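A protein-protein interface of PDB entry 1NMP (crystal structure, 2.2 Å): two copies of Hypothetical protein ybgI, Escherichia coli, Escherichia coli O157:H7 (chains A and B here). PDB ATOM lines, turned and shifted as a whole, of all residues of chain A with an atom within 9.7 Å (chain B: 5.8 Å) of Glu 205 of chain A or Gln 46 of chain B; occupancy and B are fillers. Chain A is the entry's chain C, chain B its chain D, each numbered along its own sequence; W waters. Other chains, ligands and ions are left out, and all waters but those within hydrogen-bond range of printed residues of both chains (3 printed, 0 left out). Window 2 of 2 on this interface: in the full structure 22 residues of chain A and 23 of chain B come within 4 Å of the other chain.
The side-chain amide oxygen of Gln 206 of chain A sits close to the side-chain sulfur of Met 78 of chain B (3.7 Å). The guanidinium group (NH2) of Arg 82 of chain B lies within salt-bridge range of the side-chain carboxylate (OE2) of Glu 205 of chain A (2.9 Å). The side-chain carboxylate of Glu 205 of chain A is in hydrogen-bond range of the backbone NH of Gln 46 of chain B (2.7 Å).
N of Leu 48 of chain B sits at hydrogen-bond distance from OG of Ser 45 of chain B (3.1 Å). The side-chain amide oxygen (OE1) of Gln 46 of chain B lies close to the backbone carbonyl oxygen (O) of Asn 81 of chain B (3.4 Å). The side-chain amide nitrogen (NE2) of Gln 46 of chain B lies within hydrogen-bond range of the side-chain hydroxyl (OG1) of Thr 85 of chain B, at 3.0 Å. NE2 of His 201 of chain A lies within hydrogen-bond range of OE2 of Glu 197 of chain A, at 2.9 Å. O of Ser 202 of chain A sits close to OE1 of Gln 206 of chain A, at 3.3 Å. The backbone NH of Ala 47 of chain B lies close to the side-chain hydroxyl of Ser 45 of chain B.
Among the printed residues, pairs that only touch across the chains: His 201 of chain A with Ser 45 of chain B, His 201 of chain A with Met 78 of chain B, His 201 of chain A with Arg 82 of chain B, Ser 202 of chain A with Met 78 of chain B, Glu 205 of chain A with Ser 45 of chain B and Glu 205 of chain A with Met 78 of chain B.
Glu 205 of chain A touches just these residues of chain B: Ser 45, Gln 46, Met 78 and Arg 82. Printed residues of chain A within 4 Å of Gln 46 of chain B: Glu 205 (2.7 Å). Printed residues of chain A within 4 Å of Ser 45 of chain B: His 201 and Glu 205. No residue of chain A comes within 4 Å of Ala 47 of chain B. No residue of chain A comes within 4 Å of Asn 81 of chain B. Of chain A, only His 201 and Glu 205 come within 4 Å of Arg 82 of chain B. Of the printed residues of chain B, Gln 206 of chain A touches Met 78. Printed residues of chain B within 4 Å of Ser 202 of chain A: Met 78. Ala 183 of chain A touches none of the printed residues of chain B. The nearest residue of chain A that does not touch Gln 46 of chain B is His 201 of chain A (5.9 Å).
Of the 22 printed residues of chain A, 4 touch a printed residue of chain B. Printed residues of chain A that touch a printed residue of chain B: His 201, Ser 202, Glu 205 and Gln 206. Hydrophobic or aromatic side chains of chain A within 4 Å of the printed part of chain B: His 201. Of the 12 printed residues of chain B, 4 touch a printed residue of chain A. Among the printed residues, 9 pairs touch across the chains.
No position is printed for both chains. Of the 9 pairs that touch across the chains among the printed residues, none has its exchanged pair printed and touching as well.
Water W1 lies within hydrogen-bond range of the side-chain carboxylate of Asp 180 of chain A (2.7 Å), the side-chain hydroxyl of Ser 202 of chain A (3.4 Å) and the side-chain sulfur of Met 78 of chain B (3.6 Å). Water W2 lies within hydrogen-bond range of OE1 of Glu 205 of chain A (2.7 Å), OE1 of Gln 46 of chain B (2.9 Å) and ND2 of Asn 81 of chain B (3.5 Å). Water W3 bridges the side-chain carboxylate (OE2) of Glu 205 of chain A (3.0 Å) and the backbone NH (N) of Ala 47 of chain B (3.3 Å).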
ATOM      1  N   CYS A 157      19.195 -17.377  10.754  1.00  0.00           N
ATOM      2  CA  CYS A 157      19.705 -18.482   9.967  1.00  0.00           C
ATOM      3  C   CYS A 157      20.949 -18.925  10.724  1.00  0.00           C
ATOM      4  O   CYS A 157      21.907 -18.166  10.844  1.00  0.00           O
ATOM      5  CB  CYS A 157      20.108 -18.064   8.564  1.00  0.00           C
ATOM      6  SG  CYS A 157      21.163 -19.325   7.822  1.00  0.00           S
ATOM      7  N   GLY A 158      20.937 -20.132  11.291  1.00  0.00           N
ATOM      8  CA  GLY A 158      22.144 -20.529  11.994  1.00  0.00           C
ATOM      9  C   GLY A 158      22.627 -21.905  11.604  1.00  0.00           C
ATOM     10  O   GLY A 158      23.217 -22.612  12.414  1.00  0.00           O
ATOM     11  N   ASP A 159      22.386 -22.281  10.367  1.00  0.00           N
ATOM     12  CA  ASP A 159      22.763 -23.608   9.914  1.00  0.00           C
ATOM     13  C   ASP A 159      24.226 -23.970  10.181  1.00  0.00           C
ATOM     14  O   ASP A 159      24.563 -25.149  10.380  1.00  0.00           O
ATOM     15  CB  ASP A 159      22.518 -23.743   8.412  1.00  0.00           C
ATOM     16  CG  ASP A 159      21.047 -23.524   8.027  1.00  0.00           C
ATOM     17  OD1 ASP A 159      20.140 -23.437   8.937  1.00  0.00           O
ATOM     18  OD2 ASP A 159      20.791 -23.466   6.789  1.00  0.00           O
ATOM     19  N   THR A 160      25.113 -22.989  10.124  1.00  0.00           N
ATOM     20  CA  THR A 160      26.498 -23.317  10.318  1.00  0.00           C
ATOM     21  C   THR A 160      27.179 -22.401  11.308  1.00  0.00           C
ATOM     22  O   THR A 160      28.369 -22.191  11.245  1.00  0.00           O
ATOM     23  CB  THR A 160      27.230 -23.267   8.993  1.00  0.00           C
ATOM     24  OG1 THR A 160      27.115 -21.957   8.442  1.00  0.00           O
ATOM     25  CG2 THR A 160      26.657 -24.300   7.990  1.00  0.00           C
ATOM     26  N   GLY A 161      26.430 -21.809  12.212  1.00  0.00           N
ATOM     27  CA  GLY A 161      27.077 -20.931  13.186  1.00  0.00           C
ATOM     28  C   GLY A 161      27.707 -21.708  14.341  1.00  0.00           C
ATOM     29  O   GLY A 161      27.393 -22.889  14.556  1.00  0.00           O
ATOM     30  N   ILE A 179      27.233  -8.152   5.387  1.00  0.00           N
ATOM     31  CA  ILE A 179      27.564  -9.423   6.009  1.00  0.00           C
ATOM     32  C   ILE A 179      28.896 -10.057   5.633  1.00  0.00           C
ATOM     33  O   ILE A 179      29.520 -10.630   6.513  1.00  0.00           O
ATOM     34  CB  ILE A 179      26.471 -10.483   5.810  1.00  0.00           C
ATOM     35  CG1 ILE A 179      26.832 -11.729   6.622  1.00  0.00           C
ATOM     36  CG2 ILE A 179      26.301 -10.794   4.336  1.00  0.00           C
ATOM     37  CD1 ILE A 179      25.653 -12.720   6.719  1.00  0.00           C
ATOM     38  N   ASP A 180      29.353  -9.938   4.383  1.00  0.00           N
ATOM     39  CA  ASP A 180      30.585 -10.590   3.958  1.00  0.00           C
ATOM     40  C   ASP A 180      31.759  -9.921   4.579  1.00  0.00           C
ATOM     41  O   ASP A 180      32.736 -10.567   4.937  1.00  0.00           O
ATOM     42  CB  ASP A 180      30.728 -10.573   2.412  1.00  0.00           C
ATOM     43  CG  ASP A 180      29.773 -11.577   1.737  1.00  0.00           C
ATOM     44  OD1 ASP A 180      29.036 -12.306   2.506  1.00  0.00           O
ATOM     45  OD2 ASP A 180      29.722 -11.638   0.487  1.00  0.00           O
ATOM     46  N   ALA A 183      31.968 -11.163   7.986  1.00  0.00           N
ATOM     47  CA  ALA A 183      32.590 -12.513   8.069  1.00  0.00           C
ATOM     48  C   ALA A 183      34.109 -12.503   7.894  1.00  0.00           C
ATOM     49  O   ALA A 183      34.842 -13.188   8.594  1.00  0.00           O
ATOM     50  CB  ALA A 183      31.974 -13.502   7.023  1.00  0.00           C
ATOM     51  N   GLU A 197      18.059 -12.415  -0.682  1.00  0.00           N
ATOM     52  CA  GLU A 197      18.329 -13.787  -1.088  1.00  0.00           C
ATOM     53  C   GLU A 197      19.790 -14.171  -0.871  1.00  0.00           C
ATOM     54  O   GLU A 197      20.037 -15.230  -0.279  1.00  0.00           O
ATOM     55  CB  GLU A 197      17.936 -13.991  -2.548  1.00  0.00           C
ATOM     56  CG  GLU A 197      17.942 -15.426  -3.011  1.00  0.00           C
ATOM     57  CD  GLU A 197      19.296 -15.861  -3.601  1.00  0.00           C
ATOM     58  OE1 GLU A 197      20.167 -14.984  -3.796  1.00  0.00           O
ATOM     59  OE2 GLU A 197      19.511 -17.084  -3.843  1.00  0.00           O
ATOM     60  N   GLN A 198      20.757 -13.323  -1.274  1.00  0.00           N
ATOM     61  CA  GLN A 198      22.191 -13.663  -1.141  1.00  0.00           C
ATOM     62  C   GLN A 198      22.714 -13.715   0.303  1.00  0.00           C
ATOM     63  O   GLN A 198      23.714 -14.370   0.558  1.00  0.00           O
ATOM     64  CB  GLN A 198      23.058 -12.686  -1.952  1.00  0.00           C
ATOM     65  CG  GLN A 198      22.902 -11.232  -1.492  1.00  0.00           C
ATOM     66  CD  GLN A 198      21.937 -10.481  -2.423  1.00  0.00           C
ATOM     67  OE1 GLN A 198      20.811 -10.992  -2.751  1.00  0.00           O
ATOM     68  NE2 GLN A 198      22.353  -9.268  -2.870  1.00  0.00           N
ATOM     69  N   THR A 199      22.016 -13.031   1.220  1.00  0.00           N
ATOM     70  CA  THR A 199      22.372 -12.959   2.651  1.00  0.00           C
ATOM     71  C   THR A 199      22.407 -14.352   3.279  1.00  0.00           C
ATOM     72  O   THR A 199      23.305 -14.667   4.125  1.00  0.00           O
ATOM     73  CB  THR A 199      21.324 -12.109   3.422  1.00  0.00           C
ATOM     74  OG1 THR A 199      21.048 -10.892   2.663  1.00  0.00           O
ATOM     75  CG2 THR A 199      21.878 -11.697   4.838  1.00  0.00           C
ATOM     76  N   ILE A 200      21.433 -15.199   2.888  1.00  0.00           N
ATOM     77  CA  ILE A 200      21.420 -16.495   3.468  1.00  0.00           C
ATOM     78  C   ILE A 200      22.617 -17.339   2.991  1.00  0.00           C
ATOM     79  O   ILE A 200      23.146 -18.128   3.762  1.00  0.00           O
ATOM     80  CB  ILE A 200      20.127 -17.189   3.155  1.00  0.00           C
ATOM     81  CG1 ILE A 200      18.973 -16.463   3.885  1.00  0.00           C
ATOM     82  CG2 ILE A 200      20.165 -18.622   3.701  1.00  0.00           C
ATOM     83  CD1 ILE A 200      19.082 -16.613   5.398  1.00  0.00           C
ATOM     84  N   HIS A 201      23.052 -17.209   1.735  1.00  0.00           N
ATOM     85  CA  HIS A 201      24.176 -18.009   1.322  1.00  0.00           C
ATOM     86  C   HIS A 201      25.349 -17.460   2.065  1.00  0.00           C
ATOM     87  O   HIS A 201      26.162 -18.215   2.564  1.00  0.00           O
ATOM     88  CB  HIS A 201      24.358 -17.915  -0.185  1.00  0.00           C
ATOM     89  CG  HIS A 201      23.133 -18.349  -0.936  1.00  0.00           C
ATOM     90  ND1 HIS A 201      22.546 -19.586  -0.750  1.00  0.00           N
ATOM     91  CD2 HIS A 201      22.380 -17.714  -1.856  1.00  0.00           C
ATOM     92  CE1 HIS A 201      21.484 -19.701  -1.531  1.00  0.00           C
ATOM     93  NE2 HIS A 201      21.357 -18.571  -2.214  1.00  0.00           N
ATOM     94  N   SER A 202      25.496 -16.136   2.153  1.00  0.00           N
ATOM     95  CA  SER A 202      26.633 -15.656   2.918  1.00  0.00           C
ATOM     96  C   SER A 202      26.750 -16.264   4.314  1.00  0.00           C
ATOM     97  O   SER A 202      27.859 -16.643   4.740  1.00  0.00           O
ATOM     98  CB  SER A 202      26.557 -14.154   3.017  1.00  0.00           C
ATOM     99  OG  SER A 202      26.943 -13.649   1.744  1.00  0.00           O
ATOM    100  N   ALA A 203      25.620 -16.358   5.034  1.00  0.00           N
ATOM    101  CA  ALA A 203      25.565 -16.909   6.419  1.00  0.00           C
ATOM    102  C   ALA A 203      26.054 -18.341   6.459  1.00  0.00           C
ATOM    103  O   ALA A 203      26.956 -18.697   7.222  1.00  0.00           O
ATOM    104  CB  ALA A 203      24.160 -16.890   6.912  1.00  0.00           C
ATOM    105  N   ARG A 204      25.423 -19.155   5.624  1.00  0.00           N
ATOM    106  CA  ARG A 204      25.698 -20.578   5.550  1.00  0.00           C
ATOM    107  C   ARG A 204      27.120 -20.897   5.208  1.00  0.00           C
ATOM    108  O   ARG A 204      27.776 -21.584   5.979  1.00  0.00           O
ATOM    109  CB  ARG A 204      24.773 -21.236   4.488  1.00  0.00           C
ATOM    110  CG  ARG A 204      23.261 -21.243   4.876  1.00  0.00           C
ATOM    111  CD  ARG A 204      22.346 -21.941   3.758  1.00  0.00           C
ATOM    112  NE  ARG A 204      20.976 -22.196   4.211  1.00  0.00           N
ATOM    113  CZ  ARG A 204      19.928 -22.278   3.397  1.00  0.00           C
ATOM    114  NH1 ARG A 204      20.111 -22.130   2.100  1.00  0.00           N
ATOM    115  NH2 ARG A 204      18.687 -22.440   3.881  1.00  0.00           N
ATOM    116  N   GLU A 205      27.622 -20.366   4.091  1.00  0.00           N
ATOM    117  CA  GLU A 205      28.962 -20.729   3.628  1.00  0.00           C
ATOM    118  C   GLU A 205      30.072 -20.105   4.421  1.00  0.00           C
ATOM    119  O   GLU A 205      31.197 -20.545   4.301  1.00  0.00           O
ATOM    120  CB  GLU A 205      29.114 -20.367   2.146  1.00  0.00           C
ATOM    121  CG  GLU A 205      28.040 -21.014   1.281  1.00  0.00           C
ATOM    122  CD  GLU A 205      28.110 -20.679  -0.235  1.00  0.00           C
ATOM    123  OE1 GLU A 205      29.221 -20.396  -0.751  1.00  0.00           O
ATOM    124  OE2 GLU A 205      27.044 -20.771  -0.921  1.00  0.00           O
ATOM    125  N   GLN A 206      29.784 -19.087   5.225  1.00  0.00           N
ATOM    126  CA  GLN A 206      30.835 -18.474   5.998  1.00  0.00           C
ATOM    127  C   GLN A 206      30.728 -18.839   7.451  1.00  0.00           C
ATOM    128  O   GLN A 206      31.462 -18.341   8.270  1.00  0.00           O
ATOM    129  CB  GLN A 206      30.860 -16.958   5.758  1.00  0.00           C
ATOM    130  CG  GLN A 206      31.544 -16.704   4.438  1.00  0.00           C
ATOM    131  CD  GLN A 206      31.442 -15.288   3.960  1.00  0.00           C
ATOM    132  OE1 GLN A 206      30.446 -14.600   4.222  1.00  0.00           O
ATOM    133  NE2 GLN A 206      32.459 -14.841   3.238  1.00  0.00           N
ATOM    134  N   GLY A 207      29.842 -19.756   7.783  1.00  0.00           N
ATOM    135  CA  GLY A 207      29.765 -20.197   9.170  1.00  0.00           C
ATOM    136  C   GLY A 207      29.372 -19.238  10.279  1.00  0.00           C
ATOM    137  O   GLY A 207      29.959 -19.279  11.354  1.00  0.00           O
ATOM    138  N   LEU A 208      28.400 -18.359  10.061  1.00  0.00           N
ATOM    139  CA  LEU A 208      27.989 -17.481  11.151  1.00  0.00           C
ATOM    140  C   LEU A 208      26.491 -17.508  11.308  1.00  0.00           C
ATOM    141  O   LEU A 208      25.752 -18.051  10.442  1.00  0.00           O
ATOM    142  CB  LEU A 208      28.492 -16.007  10.984  1.00  0.00           C
ATOM    143  CG  LEU A 208      27.982 -15.135   9.830  1.00  0.00           C
ATOM    144  CD1 LEU A 208      28.556 -13.761   9.876  1.00  0.00           C
ATOM    145  CD2 LEU A 208      28.408 -15.768   8.566  1.00  0.00           C
ATOM    146  N   HIS A 209      26.060 -17.006  12.462  1.00  0.00           N
ATOM    147  CA  HIS A 209      24.661 -16.881  12.796  1.00  0.00           C
ATOM    148  C   HIS A 209      24.221 -15.592  12.207  1.00  0.00           C
ATOM    149  O   HIS A 209      24.855 -14.586  12.477  1.00  0.00           O
ATOM    150  CB  HIS A 209      24.481 -16.781  14.288  1.00  0.00           C
ATOM    151  CG  HIS A 209      24.706 -18.088  14.980  1.00  0.00           C
ATOM    152  ND1 HIS A 209      23.754 -19.087  14.969  1.00  0.00           N
ATOM    153  CD2 HIS A 209      25.826 -18.631  15.526  1.00  0.00           C
ATOM    154  CE1 HIS A 209      24.274 -20.199  15.483  1.00  0.00           C
ATOM    155  NE2 HIS A 209      25.529 -19.949  15.825  1.00  0.00           N
ATOM    156  N   PHE A 210      23.131 -15.599  11.433  1.00  0.00           N
ATOM    157  CA  PHE A 210      22.630 -14.380  10.855  1.00  0.00           C
ATOM    158  C   PHE A 210      21.256 -14.037  11.403  1.00  0.00           C
ATOM    159  O   PHE A 210      20.442 -14.905  11.572  1.00  0.00           O
ATOM    160  CB  PHE A 210      22.539 -14.484   9.333  1.00  0.00           C
ATOM    161  CG  PHE A 210      21.873 -13.304   8.742  1.00  0.00           C
ATOM    162  CD1 PHE A 210      22.517 -12.048   8.740  1.00  0.00           C
ATOM    163  CD2 PHE A 210      20.574 -13.407   8.215  1.00  0.00           C
ATOM    164  CE1 PHE A 210      21.870 -10.914   8.215  1.00  0.00           C
ATOM    165  CE2 PHE A 210      19.952 -12.274   7.705  1.00  0.00           C
ATOM    166  CZ  PHE A 210      20.611 -11.021   7.702  1.00  0.00           C
ATOM    167  N   ALA B  44      23.633 -20.220  -7.900  1.00  0.00           N
ATOM    168  CA  ALA B  44      24.817 -21.098  -7.908  1.00  0.00           C
ATOM    169  C   ALA B  44      25.476 -21.058  -6.497  1.00  0.00           C
ATOM    170  O   ALA B  44      26.632 -20.635  -6.376  1.00  0.00           O
ATOM    171  CB  ALA B  44      25.812 -20.612  -8.972  1.00  0.00           C
ATOM    172  N   SER B  45      24.772 -21.553  -5.457  1.00  0.00           N
ATOM    173  CA  SER B  45      25.279 -21.507  -4.087  1.00  0.00           C
ATOM    174  C   SER B  45      26.349 -22.609  -3.909  1.00  0.00           C
ATOM    175  O   SER B  45      26.510 -23.372  -4.820  1.00  0.00           O
ATOM    176  CB  SER B  45      24.095 -21.720  -3.141  1.00  0.00           C
ATOM    177  OG  SER B  45      23.637 -23.073  -3.257  1.00  0.00           O
ATOM    178  N   GLN B  46      27.081 -22.723  -2.781  1.00  0.00           N
ATOM    179  CA  GLN B  46      28.030 -23.826  -2.701  1.00  0.00           C
ATOM    180  C   GLN B  46      27.237 -25.143  -2.603  1.00  0.00           C
ATOM    181  O   GLN B  46      27.654 -26.197  -3.128  1.00  0.00           O
ATOM    182  CB  GLN B  46      28.923 -23.708  -1.473  1.00  0.00           C
ATOM    183  CG  GLN B  46      29.914 -24.890  -1.318  1.00  0.00           C
ATOM    184  CD  GLN B  46      31.098 -24.747  -2.296  1.00  0.00           C
ATOM    185  OE1 GLN B  46      31.683 -23.659  -2.430  1.00  0.00           O
ATOM    186  NE2 GLN B  46      31.450 -25.817  -2.949  1.00  0.00           N
ATOM    187  N   ALA B  47      26.063 -25.100  -1.998  1.00  0.00           N
ATOM    188  CA  ALA B  47      25.271 -26.325  -1.862  1.00  0.00           C
ATOM    189  C   ALA B  47      24.827 -26.856  -3.186  1.00  0.00           C
ATOM    190  O   ALA B  47      24.882 -28.083  -3.396  1.00  0.00           O
ATOM    191  CB  ALA B  47      24.075 -26.076  -0.991  1.00  0.00           C
ATOM    192  N   LEU B  48      24.380 -26.009  -4.119  1.00  0.00           N
ATOM    193  CA  LEU B  48      23.966 -26.574  -5.458  1.00  0.00           C
ATOM    194  C   LEU B  48      25.210 -27.164  -6.107  1.00  0.00           C
ATOM    195  O   LEU B  48      25.198 -28.236  -6.654  1.00  0.00           O
ATOM    196  CB  LEU B  48      23.458 -25.462  -6.408  1.00  0.00           C
ATOM    197  CG  LEU B  48      22.238 -25.499  -7.326  1.00  0.00           C
ATOM    198  CD1 LEU B  48      22.717 -24.920  -8.621  1.00  0.00           C
ATOM    199  CD2 LEU B  48      21.634 -26.892  -7.482  1.00  0.00           C
ATOM    200  N   LEU B  49      26.295 -26.407  -6.051  1.00  0.00           N
ATOM    201  CA  LEU B  49      27.564 -26.846  -6.655  1.00  0.00           C
ATOM    202  C   LEU B  49      27.958 -28.206  -6.131  1.00  0.00           C
ATOM    203  O   LEU B  49      28.181 -29.114  -6.919  1.00  0.00           O
ATOM    204  CB  LEU B  49      28.668 -25.802  -6.411  1.00  0.00           C
ATOM    205  CG  LEU B  49      29.120 -24.868  -7.549  1.00  0.00           C
ATOM    206  CD1 LEU B  49      27.981 -24.551  -8.509  1.00  0.00           C
ATOM    207  CD2 LEU B  49      29.692 -23.576  -6.959  1.00  0.00           C
ATOM    208  N   ASP B  50      28.002 -28.380  -4.813  1.00  0.00           N
ATOM    209  CA  ASP B  50      28.354 -29.710  -4.250  1.00  0.00           C
ATOM    210  C   ASP B  50      27.353 -30.760  -4.805  1.00  0.00           C
ATOM    211  O   ASP B  50      27.746 -31.894  -5.068  1.00  0.00           O
ATOM    212  CB  ASP B  50      28.294 -29.661  -2.731  1.00  0.00           C
ATOM    213  CG  ASP B  50      29.412 -28.805  -2.128  1.00  0.00           C
ATOM    214  OD1 ASP B  50      30.325 -28.374  -2.894  1.00  0.00           O
ATOM    215  OD2 ASP B  50      29.407 -28.568  -0.880  1.00  0.00           O
ATOM    216  N   GLU B  51      26.069 -30.400  -5.009  1.00  0.00           N
ATOM    217  CA  GLU B  51      25.144 -31.375  -5.549  1.00  0.00           C
ATOM    218  C   GLU B  51      25.539 -31.748  -6.965  1.00  0.00           C
ATOM    219  O   GLU B  51      25.529 -32.948  -7.331  1.00  0.00           O
ATOM    220  CB  GLU B  51      23.713 -30.864  -5.575  1.00  0.00           C
ATOM    221  CG  GLU B  51      22.909 -31.220  -4.380  1.00  0.00           C
ATOM    222  CD  GLU B  51      22.851 -32.732  -4.164  1.00  0.00           C
ATOM    223  OE1 GLU B  51      22.059 -33.412  -4.874  1.00  0.00           O
ATOM    224  OE2 GLU B  51      23.627 -33.226  -3.297  1.00  0.00           O
ATOM    225  N   MET B  78      34.152 -17.124  -0.196  1.00  0.00           N
ATOM    226  CA  MET B  78      33.083 -17.875  -0.921  1.00  0.00           C
ATOM    227  C   MET B  78      33.268 -18.095  -2.412  1.00  0.00           C
ATOM    228  O   MET B  78      32.968 -19.209  -2.926  1.00  0.00           O
ATOM    229  CB  MET B  78      31.761 -17.135  -0.753  1.00  0.00           C
ATOM    230  CG  MET B  78      31.225 -17.156   0.686  1.00  0.00           C
ATOM    231  SD  MET B  78      29.732 -16.152   0.905  1.00  0.00           S
ATOM    232  CE  MET B  78      28.397 -16.938  -0.313  1.00  0.00           C
ATOM    233  N   ASN B  81      35.769 -20.656  -3.103  1.00  0.00           N
ATOM    234  CA  ASN B  81      35.304 -22.042  -2.934  1.00  0.00           C
ATOM    235  C   ASN B  81      34.372 -22.452  -4.054  1.00  0.00           C
ATOM    236  O   ASN B  81      34.399 -23.574  -4.531  1.00  0.00           O
ATOM    237  CB  ASN B  81      34.551 -22.178  -1.626  1.00  0.00           C
ATOM    238  CG  ASN B  81      35.407 -21.865  -0.432  1.00  0.00           C
ATOM    239  OD1 ASN B  81      36.554 -22.206  -0.420  1.00  0.00           O
ATOM    240  ND2 ASN B  81      34.821 -21.244   0.612  1.00  0.00           N
ATOM    241  N   ARG B  82      33.515 -21.542  -4.473  1.00  0.00           N
ATOM    242  CA  ARG B  82      32.588 -21.815  -5.525  1.00  0.00           C
ATOM    243  C   ARG B  82      33.311 -21.999  -6.866  1.00  0.00           C
ATOM    244  O   ARG B  82      33.050 -22.934  -7.601  1.00  0.00           O
ATOM    245  CB  ARG B  82      31.650 -20.641  -5.567  1.00  0.00           C
ATOM    246  CG  ARG B  82      30.606 -20.616  -4.420  1.00  0.00           C
ATOM    247  CD  ARG B  82      29.956 -19.200  -4.328  1.00  0.00           C
ATOM    248  NE  ARG B  82      28.767 -19.260  -3.475  1.00  0.00           N
ATOM    249  CZ  ARG B  82      27.742 -18.401  -3.550  1.00  0.00           C
ATOM    250  NH1 ARG B  82      27.789 -17.439  -4.448  1.00  0.00           N
ATOM    251  NH2 ARG B  82      26.663 -18.492  -2.733  1.00  0.00           N
ATOM    252  N   THR B  85      35.440 -25.303  -6.985  1.00  0.00           N
ATOM    253  CA  THR B  85      34.566 -26.486  -7.173  1.00  0.00           C
ATOM    254  C   THR B  85      34.148 -26.638  -8.649  1.00  0.00           C
ATOM    255  O   THR B  85      34.028 -27.715  -9.164  1.00  0.00           O
ATOM    256  CB  THR B  85      33.329 -26.331  -6.338  1.00  0.00           C
ATOM    257  OG1 THR B  85      33.688 -26.230  -4.945  1.00  0.00           O
ATOM    258  CG2 THR B  85      32.395 -27.539  -6.499  1.00  0.00           C
HETATM  259  O   HOH W   1      28.709 -13.469  -1.187  1.00  0.00           O
HETATM  260  O   HOH W   2      31.491 -21.742  -0.279  1.00  0.00           O
HETATM  261  O   HOH W   3      25.164 -22.764   0.221  1.00  0.00           O
